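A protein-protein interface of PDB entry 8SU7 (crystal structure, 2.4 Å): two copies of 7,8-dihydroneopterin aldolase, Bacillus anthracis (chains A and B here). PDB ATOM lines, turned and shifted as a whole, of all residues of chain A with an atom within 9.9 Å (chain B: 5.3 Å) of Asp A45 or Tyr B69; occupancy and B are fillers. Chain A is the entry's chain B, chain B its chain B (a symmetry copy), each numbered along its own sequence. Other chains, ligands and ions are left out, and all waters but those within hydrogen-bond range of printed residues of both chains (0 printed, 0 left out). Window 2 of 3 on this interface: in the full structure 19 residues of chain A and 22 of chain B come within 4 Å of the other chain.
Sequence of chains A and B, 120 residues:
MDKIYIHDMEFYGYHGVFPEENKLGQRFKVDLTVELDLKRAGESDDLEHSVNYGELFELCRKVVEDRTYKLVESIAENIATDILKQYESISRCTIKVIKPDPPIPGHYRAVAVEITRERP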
ATOM      1  N   LEU A  38     -17.051  -8.500  -5.530  1.00  0.00           N
ATOM      2  CA  LEU A  38     -16.433  -7.717  -6.591  1.00  0.00           C
ATOM      3  C   LEU A  38     -17.440  -6.886  -7.376  1.00  0.00           C
ATOM      4  O   LEU A  38     -17.089  -6.335  -8.425  1.00  0.00           O
ATOM      5  CB  LEU A  38     -15.653  -8.637  -7.531  1.00  0.00           C
ATOM      6  CG  LEU A  38     -14.320  -9.144  -6.976  1.00  0.00           C
ATOM      7  CD1 LEU A  38     -13.734 -10.251  -7.831  1.00  0.00           C
ATOM      8  CD2 LEU A  38     -13.333  -7.982  -6.851  1.00  0.00           C
ATOM      9  N   LYS A  39     -18.675  -6.763  -6.889  1.00  0.00           N
ATOM     10  CA  LYS A  39     -19.659  -5.951  -7.597  1.00  0.00           C
ATOM     11  C   LYS A  39     -19.245  -4.486  -7.622  1.00  0.00           C
ATOM     12  O   LYS A  39     -19.370  -3.815  -8.653  1.00  0.00           O
ATOM     13  CB  LYS A  39     -21.031  -6.102  -6.944  1.00  0.00           C
ATOM     14  CG  LYS A  39     -22.184  -5.636  -7.823  1.00  0.00           C
ATOM     15  CD  LYS A  39     -23.519  -5.754  -7.102  1.00  0.00           C
ATOM     16  CE  LYS A  39     -24.569  -6.394  -7.996  1.00  0.00           C
ATOM     17  NZ  LYS A  39     -25.320  -7.476  -7.292  1.00  0.00           N
ATOM     18  N   ARG A  40     -18.743  -3.971  -6.497  1.00  0.00           N
ATOM     19  CA  ARG A  40     -18.351  -2.567  -6.441  1.00  0.00           C
ATOM     20  C   ARG A  40     -17.207  -2.262  -7.399  1.00  0.00           C
ATOM     21  O   ARG A  40     -17.113  -1.143  -7.915  1.00  0.00           O
ATOM     22  CB  ARG A  40     -17.966  -2.194  -5.008  1.00  0.00           C
ATOM     23  CG  ARG A  40     -19.052  -2.501  -3.981  1.00  0.00           C
ATOM     24  CD  ARG A  40     -18.703  -1.960  -2.599  1.00  0.00           C
ATOM     25  NE  ARG A  40     -17.423  -2.460  -2.110  1.00  0.00           N
ATOM     26  CZ  ARG A  40     -17.247  -3.642  -1.536  1.00  0.00           C
ATOM     27  NH1 ARG A  40     -18.249  -4.493  -1.379  1.00  0.00           N
ATOM     28  NH2 ARG A  40     -16.034  -3.982  -1.109  1.00  0.00           N
ATOM     29  N   ALA A  41     -16.334  -3.239  -7.659  1.00  0.00           N
ATOM     30  CA  ALA A  41     -15.244  -3.019  -8.603  1.00  0.00           C
ATOM     31  C   ALA A  41     -15.762  -3.001 -10.036  1.00  0.00           C
ATOM     32  O   ALA A  41     -15.414  -2.112 -10.823  1.00  0.00           O
ATOM     33  CB  ALA A  41     -14.180  -4.103  -8.429  1.00  0.00           C
ATOM     34  N   GLY A  42     -16.601  -3.975 -10.393  1.00  0.00           N
ATOM     35  CA  GLY A  42     -17.183  -3.989 -11.723  1.00  0.00           C
ATOM     36  C   GLY A  42     -18.173  -2.865 -11.947  1.00  0.00           C
ATOM     37  O   GLY A  42     -18.316  -2.372 -13.069  1.00  0.00           O
ATOM     38  N   GLU A  43     -18.870  -2.448 -10.890  1.00  0.00           N
ATOM     39  CA  GLU A  43     -19.767  -1.306 -11.004  1.00  0.00           C
ATOM     40  C   GLU A  43     -18.992  -0.036 -11.336  1.00  0.00           C
ATOM     41  O   GLU A  43     -19.442   0.782 -12.145  1.00  0.00           O
ATOM     42  CB  GLU A  43     -20.518  -1.113  -9.688  1.00  0.00           C
ATOM     43  CG  GLU A  43     -21.855  -1.820  -9.582  1.00  0.00           C
ATOM     44  CD  GLU A  43     -22.540  -1.543  -8.252  1.00  0.00           C
ATOM     45  OE1 GLU A  43     -21.952  -0.823  -7.416  1.00  0.00           O
ATOM     46  OE2 GLU A  43     -23.664  -2.043  -8.041  1.00  0.00           O
ATOM     47  N   SER A  44     -17.821   0.142 -10.721  1.00  0.00           N
ATOM     48  CA  SER A  44     -17.091   1.400 -10.799  1.00  0.00           C
ATOM     49  C   SER A  44     -15.873   1.352 -11.711  1.00  0.00           C
ATOM     50  O   SER A  44     -15.359   2.414 -12.077  1.00  0.00           O
ATOM     51  CB  SER A  44     -16.624   1.817  -9.398  1.00  0.00           C
ATOM     52  OG  SER A  44     -15.544   1.007  -8.955  1.00  0.00           O
ATOM     53  N   ASP A  45     -15.402   0.162 -12.084  1.00  0.00           N
ATOM     54  CA  ASP A  45     -14.201   0.023 -12.909  1.00  0.00           C
ATOM     55  C   ASP A  45     -12.980   0.632 -12.220  1.00  0.00           C
ATOM     56  O   ASP A  45     -12.102   1.206 -12.866  1.00  0.00           O
ATOM     57  CB  ASP A  45     -14.405   0.632 -14.299  1.00  0.00           C
ATOM     58  CG  ASP A  45     -13.579  -0.059 -15.370  1.00  0.00           C
ATOM     59  OD1 ASP A  45     -13.261  -1.256 -15.209  1.00  0.00           O
ATOM     60  OD2 ASP A  45     -13.254   0.592 -16.384  1.00  0.00           O
ATOM     61  N   ASP A  46     -12.917   0.492 -10.895  1.00  0.00           N
ATOM     62  CA  ASP A  46     -11.866   1.095 -10.080  1.00  0.00           C
ATOM     63  C   ASP A  46     -11.138  -0.001  -9.314  1.00  0.00           C
ATOM     64  O   ASP A  46     -11.762  -0.755  -8.560  1.00  0.00           O
ATOM     65  CB  ASP A  46     -12.468   2.106  -9.103  1.00  0.00           C
ATOM     66  CG  ASP A  46     -11.646   3.374  -8.997  1.00  0.00           C
ATOM     67  OD1 ASP A  46     -10.408   3.265  -8.879  1.00  0.00           O
ATOM     68  OD2 ASP A  46     -12.236   4.476  -9.038  1.00  0.00           O
ATOM     69  N   LEU A  47      -9.817  -0.082  -9.502  1.00  0.00           N
ATOM     70  CA  LEU A  47      -9.066  -1.233  -9.012  1.00  0.00           C
ATOM     71  C   LEU A  47      -9.018  -1.285  -7.490  1.00  0.00           C
ATOM     72  O   LEU A  47      -8.889  -2.376  -6.922  1.00  0.00           O
ATOM     73  CB  LEU A  47      -7.653  -1.215  -9.598  1.00  0.00           C
ATOM     74  CG  LEU A  47      -6.660  -2.265  -9.098  1.00  0.00           C
ATOM     75  CD1 LEU A  47      -7.192  -3.677  -9.246  1.00  0.00           C
ATOM     76  CD2 LEU A  47      -5.318  -2.125  -9.843  1.00  0.00           C
ATOM     77  N   GLU A  48      -9.134  -0.135  -6.808  1.00  0.00           N
ATOM     78  CA  GLU A  48      -9.145  -0.145  -5.341  1.00  0.00           C
ATOM     79  C   GLU A  48     -10.395  -0.801  -4.756  1.00  0.00           C
ATOM     80  O   GLU A  48     -10.411  -1.084  -3.556  1.00  0.00           O
ATOM     81  CB  GLU A  48      -8.919   1.254  -4.733  1.00  0.00           C
ATOM     82  CG  GLU A  48     -10.090   2.198  -4.862  1.00  0.00           C
ATOM     83  CD  GLU A  48     -10.258   3.118  -3.638  1.00  0.00           C
ATOM     84  OE1 GLU A  48      -9.328   3.204  -2.792  1.00  0.00           O
ATOM     85  OE2 GLU A  48     -11.317   3.783  -3.540  1.00  0.00           O
ATOM     86  N   HIS A  49     -11.443  -1.020  -5.546  1.00  0.00           N
ATOM     87  CA  HIS A  49     -12.583  -1.813  -5.112  1.00  0.00           C
ATOM     88  C   HIS A  49     -12.415  -3.287  -5.456  1.00  0.00           C
ATOM     89  O   HIS A  49     -13.359  -4.066  -5.294  1.00  0.00           O
ATOM     90  CB  HIS A  49     -13.873  -1.202  -5.655  1.00  0.00           C
ATOM     91  CG  HIS A  49     -14.059   0.232  -5.254  1.00  0.00           C
ATOM     92  ND1 HIS A  49     -13.783   1.282  -6.100  1.00  0.00           N
ATOM     93  CD2 HIS A  49     -14.441   0.788  -4.078  1.00  0.00           C
ATOM     94  CE1 HIS A  49     -14.016   2.424  -5.476  1.00  0.00           C
ATOM     95  NE2 HIS A  49     -14.420   2.151  -4.248  1.00  0.00           N
ATOM     96  N   SER A  50     -11.215  -3.688  -5.875  1.00  0.00           N
ATOM     97  CA  SER A  50     -10.862  -5.089  -6.076  1.00  0.00           C
ATOM     98  C   SER A  50      -9.442  -5.302  -5.555  1.00  0.00           C
ATOM     99  O   SER A  50      -8.867  -4.435  -4.890  1.00  0.00           O
ATOM    100  CB  SER A  50     -10.999  -5.477  -7.554  1.00  0.00           C
ATOM    101  OG  SER A  50     -10.128  -6.545  -7.890  1.00  0.00           O
ATOM    102  N   TYR B  14      -9.096  -4.713 -25.524  1.00  0.00           N
ATOM    103  CA  TYR B  14      -8.135  -3.690 -25.135  1.00  0.00           C
ATOM    104  C   TYR B  14      -8.312  -3.245 -23.688  1.00  0.00           C
ATOM    105  O   TYR B  14      -7.824  -2.177 -23.305  1.00  0.00           O
ATOM    106  CB  TYR B  14      -8.236  -2.505 -26.096  1.00  0.00           C
ATOM    107  CG  TYR B  14      -7.863  -2.879 -27.513  1.00  0.00           C
ATOM    108  CD1 TYR B  14      -8.800  -3.427 -28.381  1.00  0.00           C
ATOM    109  CD2 TYR B  14      -6.569  -2.705 -27.976  1.00  0.00           C
ATOM    110  CE1 TYR B  14      -8.455  -3.776 -29.673  1.00  0.00           C
ATOM    111  CE2 TYR B  14      -6.215  -3.051 -29.264  1.00  0.00           C
ATOM    112  CZ  TYR B  14      -7.160  -3.588 -30.108  1.00  0.00           C
ATOM    113  OH  TYR B  14      -6.807  -3.933 -31.391  1.00  0.00           O
ATOM    114  N   HIS B  15      -8.965  -4.064 -22.869  1.00  0.00           N
ATOM    115  CA  HIS B  15      -9.167  -3.752 -21.465  1.00  0.00           C
ATOM    116  C   HIS B  15      -7.849  -3.863 -20.700  1.00  0.00           C
ATOM    117  O   HIS B  15      -6.919  -4.571 -21.100  1.00  0.00           O
ATOM    118  CB  HIS B  15     -10.208  -4.706 -20.861  1.00  0.00           C
ATOM    119  CG  HIS B  15     -11.384  -4.979 -21.758  1.00  0.00           C
ATOM    120  ND1 HIS B  15     -12.647  -4.490 -21.501  1.00  0.00           N
ATOM    121  CD2 HIS B  15     -11.492  -5.703 -22.901  1.00  0.00           C
ATOM    122  CE1 HIS B  15     -13.475  -4.881 -22.454  1.00  0.00           C
ATOM    123  NE2 HIS B  15     -12.798  -5.615 -23.318  1.00  0.00           N
ATOM    124  N   GLY B  16      -7.777  -3.149 -19.592  1.00  0.00           N
ATOM    125  CA  GLY B  16      -6.605  -3.169 -18.742  1.00  0.00           C
ATOM    126  C   GLY B  16      -6.433  -1.845 -18.032  1.00  0.00           C
ATOM    127  O   GLY B  16      -6.938  -0.807 -18.455  1.00  0.00           O
ATOM    128  N   ASN B  22      -4.136  -0.748 -23.120  1.00  0.00           N
ATOM    129  CA  ASN B  22      -5.200  -0.199 -23.953  1.00  0.00           C
ATOM    130  C   ASN B  22      -4.733   0.009 -25.387  1.00  0.00           C
ATOM    131  O   ASN B  22      -5.536  -0.092 -26.323  1.00  0.00           O
ATOM    132  CB  ASN B  22      -5.702   1.117 -23.358  1.00  0.00           C
ATOM    133  CG  ASN B  22      -6.072   0.991 -21.890  1.00  0.00           C
ATOM    134  OD1 ASN B  22      -5.725   1.844 -21.074  1.00  0.00           O
ATOM    135  ND2 ASN B  22      -6.775  -0.080 -21.547  1.00  0.00           N
ATOM    136  N   VAL B  63     -19.527  -6.991 -25.250  1.00  0.00           N
ATOM    137  CA  VAL B  63     -19.000  -6.457 -24.001  1.00  0.00           C
ATOM    138  C   VAL B  63     -17.479  -6.528 -23.985  1.00  0.00           C
ATOM    139  O   VAL B  63     -16.811  -5.636 -23.452  1.00  0.00           O
ATOM    140  CB  VAL B  63     -19.624  -7.194 -22.803  1.00  0.00           C
ATOM    141  CG1 VAL B  63     -19.165  -6.571 -21.493  1.00  0.00           C
ATOM    142  CG2 VAL B  63     -21.146  -7.176 -22.898  1.00  0.00           C
ATOM    143  N   ARG B  67     -16.098  -2.760 -26.380  1.00  0.00           N
ATOM    144  CA  ARG B  67     -15.916  -1.852 -25.260  1.00  0.00           C
ATOM    145  C   ARG B  67     -14.510  -2.014 -24.702  1.00  0.00           C
ATOM    146  O   ARG B  67     -13.821  -3.002 -24.971  1.00  0.00           O
ATOM    147  CB  ARG B  67     -16.936  -2.123 -24.147  1.00  0.00           C
ATOM    148  CG  ARG B  67     -18.229  -2.769 -24.611  1.00  0.00           C
ATOM    149  CD  ARG B  67     -19.374  -2.450 -23.658  1.00  0.00           C
ATOM    150  NE  ARG B  67     -20.206  -1.362 -24.157  1.00  0.00           N
ATOM    151  CZ  ARG B  67     -21.365  -1.525 -24.779  1.00  0.00           C
ATOM    152  NH1 ARG B  67     -21.873  -2.728 -24.995  1.00  0.00           N
ATOM    153  NH2 ARG B  67     -22.031  -0.454 -25.202  1.00  0.00           N
ATOM    154  N   THR B  68     -14.088  -1.029 -23.909  1.00  0.00           N
ATOM    155  CA  THR B  68     -12.775  -1.047 -23.274  1.00  0.00           C
ATOM    156  C   THR B  68     -12.931  -0.577 -21.838  1.00  0.00           C
ATOM    157  O   THR B  68     -13.281   0.584 -21.600  1.00  0.00           O
ATOM    158  CB  THR B  68     -11.793  -0.140 -24.025  1.00  0.00           C
ATOM    159  OG1 THR B  68     -11.672  -0.578 -25.384  1.00  0.00           O
ATOM    160  CG2 THR B  68     -10.421  -0.163 -23.365  1.00  0.00           C
ATOM    161  N   TYR B  69     -12.663  -1.465 -20.890  1.00  0.00           N
ATOM    162  CA  TYR B  69     -12.719  -1.146 -19.472  1.00  0.00           C
ATOM    163  C   TYR B  69     -11.326  -1.230 -18.859  1.00  0.00           C
ATOM    164  O   TYR B  69     -10.365  -1.678 -19.487  1.00  0.00           O
ATOM    165  CB  TYR B  69     -13.647  -2.115 -18.731  1.00  0.00           C
ATOM    166  CG  TYR B  69     -15.078  -2.160 -19.215  1.00  0.00           C
ATOM    167  CD1 TYR B  69     -15.387  -2.559 -20.499  1.00  0.00           C
ATOM    168  CD2 TYR B  69     -16.125  -1.821 -18.370  1.00  0.00           C
ATOM    169  CE1 TYR B  69     -16.693  -2.610 -20.931  1.00  0.00           C
ATOM    170  CE2 TYR B  69     -17.437  -1.873 -18.797  1.00  0.00           C
ATOM    171  CZ  TYR B  69     -17.713  -2.264 -20.080  1.00  0.00           C
ATOM    172  OH  TYR B  69     -19.018  -2.315 -20.511  1.00  0.00           O
ATOM    173  N   LYS B  70     -11.229  -0.809 -17.597  1.00  0.00           N
ATOM    174  CA  LYS B  70      -9.984  -0.998 -16.860  1.00  0.00           C
ATOM    175  C   LYS B  70      -9.910  -2.400 -16.271  1.00  0.00           C
ATOM    176  O   LYS B  70      -8.892  -3.090 -16.402  1.00  0.00           O
ATOM    177  CB  LYS B  70      -9.861   0.037 -15.740  1.00  0.00           C
ATOM    178  CG  LYS B  70     -10.216   1.459 -16.132  1.00  0.00           C
ATOM    179  CD  LYS B  70      -9.933   2.430 -14.985  1.00  0.00           C
ATOM    180  CE  LYS B  70     -11.046   3.456 -14.819  1.00  0.00           C
ATOM    181  NZ  LYS B  70     -11.662   3.856 -16.121  1.00  0.00           N
ATOM    182  N   LEU B  71     -10.987  -2.842 -15.630  1.00  0.00           N
ATOM    183  CA  LEU B  71     -11.001  -4.104 -14.910  1.00  0.00           C
ATOM    184  C   LEU B  71     -11.766  -5.164 -15.690  1.00  0.00           C
ATOM    185  O   LEU B  71     -12.800  -4.877 -16.303  1.00  0.00           O
ATOM    186  CB  LEU B  71     -11.667  -3.923 -13.545  1.00  0.00           C
ATOM    187  CG  LEU B  71     -11.256  -2.717 -12.702  1.00  0.00           C
ATOM    188  CD1 LEU B  71     -11.956  -2.753 -11.344  1.00  0.00           C
ATOM    189  CD2 LEU B  71      -9.750  -2.681 -12.531  1.00  0.00           C
ATOM    190  N   SER B  74     -15.316  -5.549 -14.494  1.00  0.00           N
ATOM    191  CA  SER B  74     -16.390  -4.813 -15.151  1.00  0.00           C
ATOM    192  C   SER B  74     -16.925  -5.571 -16.355  1.00  0.00           C
ATOM    193  O   SER B  74     -18.101  -5.421 -16.712  1.00  0.00           O
ATOM    194  CB  SER B  74     -15.887  -3.434 -15.576  1.00  0.00           C
ATOM    195  OG  SER B  74     -15.473  -2.673 -14.453  1.00  0.00           O
ATOM    196  N   ILE B  75     -16.072  -6.372 -16.999  1.00  0.00           N
ATOM    197  CA  ILE B  75     -16.542  -7.236 -18.069  1.00  0.00           C
ATOM    198  C   ILE B  75     -17.528  -8.245 -17.511  1.00  0.00           C
ATOM    199  O   ILE B  75     -18.663  -8.322 -17.965  1.00  0.00           O
ATOM    200  CB  ILE B  75     -15.371  -7.906 -18.807  1.00  0.00           C
ATOM    201  CG1 ILE B  75     -14.188  -6.942 -18.898  1.00  0.00           C
ATOM    202  CG2 ILE B  75     -15.808  -8.336 -20.194  1.00  0.00           C
ATOM    203  CD1 ILE B  75     -13.059  -7.398 -19.793  1.00  0.00           C
ATOM    204  N   ASN B  78     -20.970  -6.504 -16.506  1.00  0.00           N
ATOM    205  CA  ASN B  78     -21.803  -6.039 -17.610  1.00  0.00           C
ATOM    206  C   ASN B  78     -22.337  -7.202 -18.434  1.00  0.00           C
ATOM    207  O   ASN B  78     -23.470  -7.152 -18.928  1.00  0.00           O
ATOM    208  CB  ASN B  78     -21.020  -5.059 -18.482  1.00  0.00           C
ATOM    209  CG  ASN B  78     -20.932  -3.663 -17.866  1.00  0.00           C
ATOM    210  OD1 ASN B  78     -20.268  -2.782 -18.406  1.00  0.00           O
ATOM    211  ND2 ASN B  78     -21.598  -3.461 -16.733  1.00  0.00           N
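CD1 of Leu B71 touches O of Ala A41 (3.6 Å).
OG of Ser B74 touches O of Ala A41, 3.7 Å away.
Tyr B69 touches Asp A45 (CA to OD2, 3.6 Å).
Asp A46 touches Leu B71.
Leu B71 touches Leu A47 (CD2 to CA, 3.9 Å).
OG of Ser B74 lies within hydrogen-bond range of O of Gly A42 (3.2 Å).
The side-chain carboxylate (OD2) of Asp A45 is in salt-bridge range of the side-chain amino group (NZ) of Lys B70 (3.6 Å).
The backbone NH (N) of Leu B71 lies within hydrogen-bond range of the side-chain carboxylate (OD1) of Asp A45.
The side-chain hydroxyl (OG) of Ser B74 is in hydrogen-bond range of the side-chain carboxylate (OD1) of Asp A45, at 2.7 Å.
Hydrophobic or aromatic side chains of chain B that line the printed part of chain A: Tyr B69 and Leu B71.
Hydrophobic or aromatic side chains of chain A that line the printed part of chain B: Ala A41 and Leu A47.
Among the printed residues, 9 pairs touch across the chains.
The side-chain hydroxyl (OG) of Ser A44 sits close to the backbone NH (N) of Asp A46.
A ring nitrogen (ND1) of His B15 lies within hydrogen-bond range of the backbone NH (N) of Tyr B69 (3.1 Å).
The backbone NH (N) of Gly B16 lies within hydrogen-bond range of the backbone carbonyl oxygen (O) of Tyr B69, at 3.0 Å.
N of Gly B16 lies close to O of Lys B70.
OH of Tyr B69 is in hydrogen-bond range of OD1 of Asn B78 (2.5 Å).
No position is printed for both chains.
Of the 9 pairs that touch across the chains among the printed residues, none has its exchanged pair printed and touching as well.
Printed residues of chain A within 4 Å of Tyr B69: Asp A45 (3.6 Å).
No residue of chain A comes within 4 Å of His B15.
No residue of chain A comes within 4 Å of Thr B68.
Of chain A, only Ala A41 (3.6 Å), Asp A45 (2.8 Å), Asp A46 (3.4 Å) and Leu A47 (3.9 Å) come within 4 Å of Leu B71.
Of chain A, only Ala A41, Gly A42 and Asp A45 come within 4 Å of Ser B74.
Of the printed residues of chain B, Gly A42 touches Ser B74.
Printed residues of chain B within 4 Å of Ala A41: Leu B71 (3.6 Å) and Ser B74 (3.7 Å).
Ile B75 touches none of the printed residues of chain A.
Asn B78 touches none of the printed residues of chain A.
The nearest residue of chain B that does not touch Asp A45 is Thr B68 (5.2 Å).
The nearest residue of chain A that does not touch Tyr B69 is Gly A42 (5.8 Å).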
